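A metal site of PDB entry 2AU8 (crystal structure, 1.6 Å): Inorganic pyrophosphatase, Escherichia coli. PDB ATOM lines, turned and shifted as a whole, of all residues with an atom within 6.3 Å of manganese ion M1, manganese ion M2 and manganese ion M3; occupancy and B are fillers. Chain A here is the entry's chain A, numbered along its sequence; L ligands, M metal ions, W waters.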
ATOM      1  N   GLU A  20      16.863  23.860   5.229  1.00  0.00           N
ATOM      2  CA  GLU A  20      15.730  24.242   4.424  1.00  0.00           C
ATOM      3  C   GLU A  20      14.437  24.222   5.201  1.00  0.00           C
ATOM      4  O   GLU A  20      13.570  25.079   4.952  1.00  0.00           O
ATOM      5  CB  GLU A  20      15.505  23.271   3.250  1.00  0.00           C
ATOM      6  CG  GLU A  20      16.647  23.364   2.262  1.00  0.00           C
ATOM      7  CD  GLU A  20      16.687  22.373   1.141  1.00  0.00           C
ATOM      8  OE1 GLU A  20      16.485  21.170   1.479  1.00  0.00           O
ATOM      9  OE2 GLU A  20      16.935  22.737  -0.028  1.00  0.00           O
ATOM     10  N   LYS A  29       7.481  22.199   2.476  1.00  0.00           N
ATOM     11  CA  LYS A  29       8.721  21.742   1.956  1.00  0.00           C
ATOM     12  C   LYS A  29       9.414  22.810   1.134  1.00  0.00           C
ATOM     13  O   LYS A  29       9.016  22.988  -0.040  1.00  0.00           O
ATOM     14  CB  LYS A  29       8.410  20.533   1.058  1.00  0.00           C
ATOM     15  CG  LYS A  29       9.379  19.418   1.222  1.00  0.00           C
ATOM     16  CD  LYS A  29      10.479  19.403   0.259  1.00  0.00           C
ATOM     17  CE  LYS A  29      11.396  18.167   0.462  1.00  0.00           C
ATOM     18  NZ  LYS A  29      12.744  18.577  -0.088  1.00  0.00           N
ATOM     19  N   GLU A  31      12.934  24.378  -0.714  1.00  0.00           N
ATOM     20  CA  GLU A  31      14.146  23.930  -1.353  1.00  0.00           C
ATOM     21  C   GLU A  31      14.900  25.180  -1.730  1.00  0.00           C
ATOM     22  O   GLU A  31      14.350  26.178  -2.120  1.00  0.00           O
ATOM     23  CB  GLU A  31      13.906  23.083  -2.584  1.00  0.00           C
ATOM     24  CG  GLU A  31      13.409  21.731  -2.228  1.00  0.00           C
ATOM     25  CD  GLU A  31      13.402  20.583  -3.205  1.00  0.00           C
ATOM     26  OE1 GLU A  31      13.206  20.851  -4.390  1.00  0.00           O
ATOM     27  OE2 GLU A  31      13.582  19.386  -2.853  1.00  0.00           O
ATOM     28  N   ARG A  43       6.668  22.108  -2.300  1.00  0.00           N
ATOM     29  CA  ARG A  43       5.435  21.462  -1.970  1.00  0.00           C
ATOM     30  C   ARG A  43       4.788  21.923  -0.666  1.00  0.00           C
ATOM     31  O   ARG A  43       5.462  22.169   0.312  1.00  0.00           O
ATOM     32  CB  ARG A  43       5.714  19.960  -1.819  1.00  0.00           C
ATOM     33  CG  ARG A  43       4.671  18.941  -2.044  1.00  0.00           C
ATOM     34  CD  ARG A  43       5.086  17.511  -2.108  1.00  0.00           C
ATOM     35  NE  ARG A  43       6.231  16.899  -1.433  1.00  0.00           N
ATOM     36  CZ  ARG A  43       7.428  16.519  -1.884  1.00  0.00           C
ATOM     37  NH1 ARG A  43       7.762  16.706  -3.156  1.00  0.00           N
ATOM     38  NH2 ARG A  43       8.382  15.962  -1.129  1.00  0.00           N
ATOM     39  N   TYR A  55      15.944  19.887   8.611  1.00  0.00           N
ATOM     40  CA  TYR A  55      16.246  19.175   7.386  1.00  0.00           C
ATOM     41  C   TYR A  55      16.889  20.094   6.361  1.00  0.00           C
ATOM     42  O   TYR A  55      16.473  21.256   6.172  1.00  0.00           O
ATOM     43  CB  TYR A  55      14.940  18.658   6.860  1.00  0.00           C
ATOM     44  CG  TYR A  55      15.076  17.806   5.621  1.00  0.00           C
ATOM     45  CD1 TYR A  55      15.520  16.491   5.717  1.00  0.00           C
ATOM     46  CD2 TYR A  55      14.759  18.335   4.367  1.00  0.00           C
ATOM     47  CE1 TYR A  55      15.661  15.685   4.607  1.00  0.00           C
ATOM     48  CE2 TYR A  55      14.898  17.508   3.249  1.00  0.00           C
ATOM     49  CZ  TYR A  55      15.343  16.191   3.373  1.00  0.00           C
ATOM     50  OH  TYR A  55      15.484  15.385   2.278  1.00  0.00           O
ATOM     51  N   GLY A  56      17.906  19.581   5.691  1.00  0.00           N
ATOM     52  CA  GLY A  56      18.574  20.361   4.673  1.00  0.00           C
ATOM     53  C   GLY A  56      19.556  19.553   3.865  1.00  0.00           C
ATOM     54  O   GLY A  56      19.338  18.379   3.589  1.00  0.00           O
ATOM     55  N   TYR A  57      20.678  20.141   3.445  1.00  0.00           N
ATOM     56  CA  TYR A  57      21.602  19.453   2.609  1.00  0.00           C
ATOM     57  C   TYR A  57      23.021  19.935   2.825  1.00  0.00           C
ATOM     58  O   TYR A  57      23.261  20.968   3.519  1.00  0.00           O
ATOM     59  CB  TYR A  57      21.191  19.704   1.155  1.00  0.00           C
ATOM     60  CG  TYR A  57      21.346  21.159   0.716  1.00  0.00           C
ATOM     61  CD1 TYR A  57      20.281  22.028   0.928  1.00  0.00           C
ATOM     62  CD2 TYR A  57      22.482  21.709   0.103  1.00  0.00           C
ATOM     63  CE1 TYR A  57      20.283  23.382   0.583  1.00  0.00           C
ATOM     64  CE2 TYR A  57      22.514  23.062  -0.258  1.00  0.00           C
ATOM     65  CZ  TYR A  57      21.434  23.883  -0.019  1.00  0.00           C
ATOM     66  OH  TYR A  57      21.471  25.195  -0.374  1.00  0.00           O
ATOM     67  N   SER A  63      23.310  13.732  -4.850  1.00  0.00           N
ATOM     68  CA  SER A  63      22.696  12.440  -4.692  1.00  0.00           C
ATOM     69  C   SER A  63      22.225  11.992  -6.060  1.00  0.00           C
ATOM     70  O   SER A  63      22.188  12.802  -6.959  1.00  0.00           O
ATOM     71  CB  SER A  63      21.470  12.401  -3.791  1.00  0.00           C
ATOM     72  OG  SER A  63      21.937  12.328  -2.437  1.00  0.00           O
ATOM     73  N   ASP A  65      19.392  11.388  -6.774  1.00  0.00           N
ATOM     74  CA  ASP A  65      18.114  11.990  -7.019  1.00  0.00           C
ATOM     75  C   ASP A  65      18.285  13.318  -7.719  1.00  0.00           C
ATOM     76  O   ASP A  65      17.361  14.081  -8.076  1.00  0.00           O
ATOM     77  CB  ASP A  65      17.433  12.093  -5.637  1.00  0.00           C
ATOM     78  CG  ASP A  65      17.817  13.274  -4.792  1.00  0.00           C
ATOM     79  OD1 ASP A  65      16.918  13.625  -3.957  1.00  0.00           O
ATOM     80  OD2 ASP A  65      18.915  13.789  -4.967  1.00  0.00           O
ATOM     81  N   ASP A  67      19.739  15.996  -6.460  1.00  0.00           N
ATOM     82  CA  ASP A  67      20.002  17.237  -5.651  1.00  0.00           C
ATOM     83  C   ASP A  67      21.061  17.029  -4.609  1.00  0.00           C
ATOM     84  O   ASP A  67      21.503  15.882  -4.363  1.00  0.00           O
ATOM     85  CB  ASP A  67      18.679  17.708  -5.064  1.00  0.00           C
ATOM     86  CG  ASP A  67      18.015  18.636  -6.104  1.00  0.00           C
ATOM     87  OD1 ASP A  67      18.752  19.554  -6.601  1.00  0.00           O
ATOM     88  OD2 ASP A  67      16.839  18.403  -6.367  1.00  0.00           O
ATOM     89  N   PRO A  68      21.601  18.014  -3.934  1.00  0.00           N
ATOM     90  CA  PRO A  68      22.586  17.709  -2.851  1.00  0.00           C
ATOM     91  C   PRO A  68      22.065  16.751  -1.811  1.00  0.00           C
ATOM     92  O   PRO A  68      20.884  16.559  -1.499  1.00  0.00           O
ATOM     93  CB  PRO A  68      22.870  19.113  -2.248  1.00  0.00           C
ATOM     94  CG  PRO A  68      22.631  20.036  -3.418  1.00  0.00           C
ATOM     95  CD  PRO A  68      21.435  19.456  -4.113  1.00  0.00           C
ATOM     96  N   VAL A  69      23.034  16.051  -1.226  1.00  0.00           N
ATOM     97  CA  VAL A  69      22.656  15.033  -0.229  1.00  0.00           C
ATOM     98  C   VAL A  69      21.987  15.660   0.971  1.00  0.00           C
ATOM     99  O   VAL A  69      22.320  16.709   1.478  1.00  0.00           O
ATOM    100  CB  VAL A  69      23.894  14.231   0.207  1.00  0.00           C
ATOM    101  CG1 VAL A  69      24.865  15.109   0.932  1.00  0.00           C
ATOM    102  CG2 VAL A  69      23.426  12.998   1.042  1.00  0.00           C
ATOM    103  N   ASP A  70      20.983  14.918   1.408  1.00  0.00           N
ATOM    104  CA  ASP A  70      20.085  15.385   2.432  1.00  0.00           C
ATOM    105  C   ASP A  70      20.538  15.034   3.824  1.00  0.00           C
ATOM    106  O   ASP A  70      21.136  13.991   4.131  1.00  0.00           O
ATOM    107  CB  ASP A  70      18.690  14.764   2.195  1.00  0.00           C
ATOM    108  CG  ASP A  70      18.207  15.117   0.805  1.00  0.00           C
ATOM    109  OD1 ASP A  70      18.313  16.299   0.512  1.00  0.00           O
ATOM    110  OD2 ASP A  70      17.781  14.150   0.198  1.00  0.00           O
ATOM    111  N   MET A  95      17.680   4.986   1.794  1.00  0.00           N
ATOM    112  CA  MET A  95      16.330   4.895   1.253  1.00  0.00           C
ATOM    113  C   MET A  95      16.384   5.374  -0.180  1.00  0.00           C
ATOM    114  O   MET A  95      17.334   6.076  -0.554  1.00  0.00           O
ATOM    115  CB  MET A  95      15.319   5.683   2.097  1.00  0.00           C
ATOM    116  CG  MET A  95      15.705   7.159   2.316  1.00  0.00           C
ATOM    117  SD  MET A  95      14.284   8.205   2.733  1.00  0.00           S
ATOM    118  CE  MET A  95      13.582   8.454   1.113  1.00  0.00           C
ATOM    119  N   ASP A  97      13.847   7.235  -3.433  1.00  0.00           N
ATOM    120  CA  ASP A  97      12.472   7.772  -3.578  1.00  0.00           C
ATOM    121  C   ASP A  97      12.213   7.777  -5.055  1.00  0.00           C
ATOM    122  O   ASP A  97      13.041   7.297  -5.815  1.00  0.00           O
ATOM    123  CB  ASP A  97      12.264   9.125  -2.909  1.00  0.00           C
ATOM    124  CG  ASP A  97      12.737  10.417  -3.445  1.00  0.00           C
ATOM    125  OD1 ASP A  97      13.484  10.425  -4.428  1.00  0.00           O
ATOM    126  OD2 ASP A  97      12.323  11.440  -2.804  1.00  0.00           O
ATOM    127  N   GLU A  98      11.072   8.295  -5.507  1.00  0.00           N
ATOM    128  CA  GLU A  98      10.823   8.217  -6.946  1.00  0.00           C
ATOM    129  C   GLU A  98      11.878   8.952  -7.754  1.00  0.00           C
ATOM    130  O   GLU A  98      11.893   8.795  -9.008  1.00  0.00           O
ATOM    131  CB  GLU A  98       9.394   8.747  -7.238  1.00  0.00           C
ATOM    132  CG  GLU A  98       9.355  10.278  -7.220  1.00  0.00           C
ATOM    133  CD  GLU A  98       9.556  10.844  -5.822  1.00  0.00           C
ATOM    134  OE1 GLU A  98       9.138  10.109  -4.882  1.00  0.00           O
ATOM    135  OE2 GLU A  98      10.105  11.956  -5.709  1.00  0.00           O
ATOM    136  N   ALA A  99      12.815   9.756  -7.195  1.00  0.00           N
ATOM    137  CA  ALA A  99      13.747  10.450  -8.099  1.00  0.00           C
ATOM    138  C   ALA A  99      15.156   9.888  -8.084  1.00  0.00           C
ATOM    139  O   ALA A  99      16.044  10.422  -8.759  1.00  0.00           O
ATOM    140  CB  ALA A  99      13.788  11.935  -7.760  1.00  0.00           C
ATOM    141  N   GLY A 100      15.421   8.810  -7.354  1.00  0.00           N
ATOM    142  CA  GLY A 100      16.782   8.269  -7.223  1.00  0.00           C
ATOM    143  C   GLY A 100      17.058   7.874  -5.770  1.00  0.00           C
ATOM    144  O   GLY A 100      16.287   8.077  -4.784  1.00  0.00           O
ATOM    145  N   GLU A 101      18.239   7.271  -5.642  1.00  0.00           N
ATOM    146  CA  GLU A 101      18.757   6.840  -4.342  1.00  0.00           C
ATOM    147  C   GLU A 101      18.760   8.141  -3.527  1.00  0.00           C
ATOM    148  O   GLU A 101      19.171   9.158  -4.122  1.00  0.00           O
ATOM    149  CB  GLU A 101      20.137   6.197  -4.350  1.00  0.00           C
ATOM    150  CG  GLU A 101      20.467   5.532  -3.017  1.00  0.00           C
ATOM    151  CD  GLU A 101      19.484   4.400  -2.754  1.00  0.00           C
ATOM    152  OE1 GLU A 101      18.839   4.027  -3.758  1.00  0.00           O
ATOM    153  OE2 GLU A 101      19.352   3.913  -1.601  1.00  0.00           O
ATOM    154  N   ASP A 102      18.320   8.009  -2.291  1.00  0.00           N
ATOM    155  CA  ASP A 102      18.079   9.278  -1.597  1.00  0.00           C
ATOM    156  C   ASP A 102      18.275   9.212  -0.099  1.00  0.00           C
ATOM    157  O   ASP A 102      17.260   9.540   0.541  1.00  0.00           O
ATOM    158  CB  ASP A 102      16.625   9.717  -1.885  1.00  0.00           C
ATOM    159  CG  ASP A 102      16.315  11.164  -1.584  1.00  0.00           C
ATOM    160  OD1 ASP A 102      17.286  11.984  -1.514  1.00  0.00           O
ATOM    161  OD2 ASP A 102      15.086  11.426  -1.435  1.00  0.00           O
ATOM    162  N   ALA A 103      19.492   8.834   0.286  1.00  0.00           N
ATOM    163  CA  ALA A 103      19.907   8.640   1.664  1.00  0.00           C
ATOM    164  C   ALA A 103      19.649   9.875   2.514  1.00  0.00           C
ATOM    165  O   ALA A 103      19.755  11.044   2.079  1.00  0.00           O
ATOM    166  CB  ALA A 103      21.390   8.313   1.779  1.00  0.00           C
ATOM    167  N   LYS A 104      19.297   9.622   3.762  1.00  0.00           N
ATOM    168  CA  LYS A 104      19.101  10.703   4.688  1.00  0.00           C
ATOM    169  C   LYS A 104      20.159  10.605   5.792  1.00  0.00           C
ATOM    170  O   LYS A 104      20.111   9.781   6.707  1.00  0.00           O
ATOM    171  CB  LYS A 104      17.707  10.684   5.291  1.00  0.00           C
ATOM    172  CG  LYS A 104      16.579  10.680   4.328  1.00  0.00           C
ATOM    173  CD  LYS A 104      16.555  11.960   3.477  1.00  0.00           C
ATOM    174  CE  LYS A 104      15.329  11.841   2.583  1.00  0.00           C
ATOM    175  NZ  LYS A 104      15.510  12.395   1.219  1.00  0.00           N
ATOM    176  N   TYR A 141       5.224  10.235   4.576  1.00  0.00           N
ATOM    177  CA  TYR A 141       4.893  11.655   4.310  1.00  0.00           C
ATOM    178  C   TYR A 141       4.377  11.915   2.903  1.00  0.00           C
ATOM    179  O   TYR A 141       3.682  12.886   2.624  1.00  0.00           O
ATOM    180  CB  TYR A 141       6.088  12.559   4.595  1.00  0.00           C
ATOM    181  CG  TYR A 141       7.208  12.779   3.628  1.00  0.00           C
ATOM    182  CD1 TYR A 141       8.106  11.856   3.151  1.00  0.00           C
ATOM    183  CD2 TYR A 141       7.358  14.098   3.170  1.00  0.00           C
ATOM    184  CE1 TYR A 141       9.098  12.192   2.257  1.00  0.00           C
ATOM    185  CE2 TYR A 141       8.338  14.451   2.284  1.00  0.00           C
ATOM    186  CZ  TYR A 141       9.202  13.495   1.835  1.00  0.00           C
ATOM    187  OH  TYR A 141      10.179  13.910   0.939  1.00  0.00           O
ATOM    188  N   LYS A 142       4.739  11.026   2.008  1.00  0.00           N
ATOM    189  CA  LYS A 142       4.251  11.167   0.644  1.00  0.00           C
ATOM    190  C   LYS A 142       3.050  10.261   0.366  1.00  0.00           C
ATOM    191  O   LYS A 142       2.659  10.013  -0.799  1.00  0.00           O
ATOM    192  CB  LYS A 142       5.347  10.839  -0.339  1.00  0.00           C
ATOM    193  CG  LYS A 142       6.587  11.747  -0.275  1.00  0.00           C
ATOM    194  CD  LYS A 142       7.540  11.164  -1.342  1.00  0.00           C
ATOM    195  CE  LYS A 142       8.876  11.732  -1.423  1.00  0.00           C
ATOM    196  NZ  LYS A 142       9.468  11.832  -2.794  1.00  0.00           N
ATOM    197  N   VAL A 150       8.308   6.224  -1.308  1.00  0.00           N
ATOM    198  CA  VAL A 150       9.546   5.951  -0.623  1.00  0.00           C
ATOM    199  C   VAL A 150       9.701   4.463  -0.233  1.00  0.00           C
ATOM    200  O   VAL A 150       8.782   3.833   0.150  1.00  0.00           O
ATOM    201  CB  VAL A 150       9.694   6.768   0.682  1.00  0.00           C
ATOM    202  CG1 VAL A 150      10.857   6.339   1.541  1.00  0.00           C
ATOM    203  CG2 VAL A 150       9.887   8.222   0.278  1.00  0.00           C
HETATM  204  P1  LIG L   1      15.045  15.984  -1.320  1.00  0.00           P
HETATM  205  O1  LIG L   1      13.886  16.506  -2.133  1.00  0.00           O
HETATM  206  O2  LIG L   1      15.154  16.609   0.041  1.00  0.00           O
HETATM  207  O3  LIG L   1      14.863  14.488  -1.237  1.00  0.00           O
HETATM  208  O4  LIG L   1      16.273  16.301  -2.145  1.00  0.00           O
HETATM  209 CL1  LG2 L   2      12.617  12.247   0.414  1.00  0.00          CL
HETATM  210 MN    MN M   1      17.073  14.130  -1.859  1.00  0.00          MN
HETATM  211 MN    MN M   2      17.047  17.654  -0.465  1.00  0.00          MN
HETATM  212 MN    MN M   3      13.528  12.872  -1.831  1.00  0.00          MN
HETATM  213 MN    MN M   4      13.403  17.506  -3.927  1.00  0.00          MN
HETATM  214  O   HOH W   1      11.990  14.401  -2.281  1.00  0.00           O
HETATM  215  O   HOH W   2      18.795  18.372  -1.498  1.00  0.00           O
HETATM  216  O   HOH W   3      18.998  14.605  -2.448  1.00  0.00           O
HETATM  217  O   HOH W   4      14.218  13.122  -4.091  1.00  0.00           O
HETATM  218  O   HOH W   5      17.318  18.756   1.414  1.00  0.00           O
HETATM  219  O   HOH W   6      16.019  19.510  -1.154  1.00  0.00           O
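The backbone carbonyl oxygen of Asp 102 lies close to the side-chain amino group of Lys 104 (3.4 Å).
OH of Tyr 55 lies close to OD2 of Asp 70 (3.3 Å).
NZ of Lys 142 lies close to OD2 of Asp 97.
The side-chain carboxylate (OD1) of Asp 97 is in hydrogen-bond range of the backbone NH (N) of Ala 99 (2.9 Å).
NZ of Lys 104 sits close to OD2 of Asp 70 (3.0 Å).
N of Asp 102 is in hydrogen-bond range of O of Met 95, 2.8 Å away.
O of Tyr 55 lies within hydrogen-bond range of N of Glu 20 (2.8 Å).
The side-chain carboxylate (OD2) of Asp 65 is in hydrogen-bond range of the backbone NH (N) of Asp 67 (2.8 Å).
Merely in contact with manganese ion M1: Lys 104 (3.9 Å).
Four residues have an atom within 4 Å of manganese ion M1: Asp 65, Asp 70, Asp 102 and Lys 104.
The nearest printed residue that does not touch manganese ion M1 is Pro 68 (4.5 Å).
Merely in contact with manganese ion M2: Tyr 55.
Within 4 Å of manganese ion M2: Tyr 55 and Asp 70.
NZ of Lys 104 touches manganese ion M3, at 3.7 Å.
The nearest printed residue that does not touch manganese ion M3 is Asp 65 (4.1 Å).
Manganese ion M1 is bound by water W3, at 2.1 Å.
Manganese ion M1 is bound by OD1 of Asp 65, 2.2 Å away.
The side-chain carboxylate (OD2) of Asp 70 is bound to manganese ion M1, at 2.2 Å.
Manganese ion M1 is bound by the side-chain carboxylate (OD1) of Asp 102 (2.2 Å).
An oxygen (O3) of LIG L1 is bound to manganese ion M1 (2.3 Å).
O4 of LIG L1 binds manganese ion M1, at 2.3 Å.
Manganese ion M2 is bound by OD1 of Asp 70 (2.1 Å), water W2 (2.2 Å), water W5 (2.2 Å), O2 of LIG L1 (2.2 Å), water W6 (2.2 Å) and O4 of LIG L1 (2.3 Å).
Manganese ion M3 is bound by OD2 of Asp 97 (2.1 Å), OD2 of Asp 102 (2.2 Å), O3 of LIG L1 (2.2 Å), water W1 (2.2 Å), water W4 (2.4 Å) and CL1 of LG2 L2 (2.5 Å).
Manganese ion M3 has six donor atoms within binding distance.
Water W5 lies within hydrogen-bond range of OE1 of Glu 20 (2.6 Å) and O of Gly 56 (3.0 Å).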
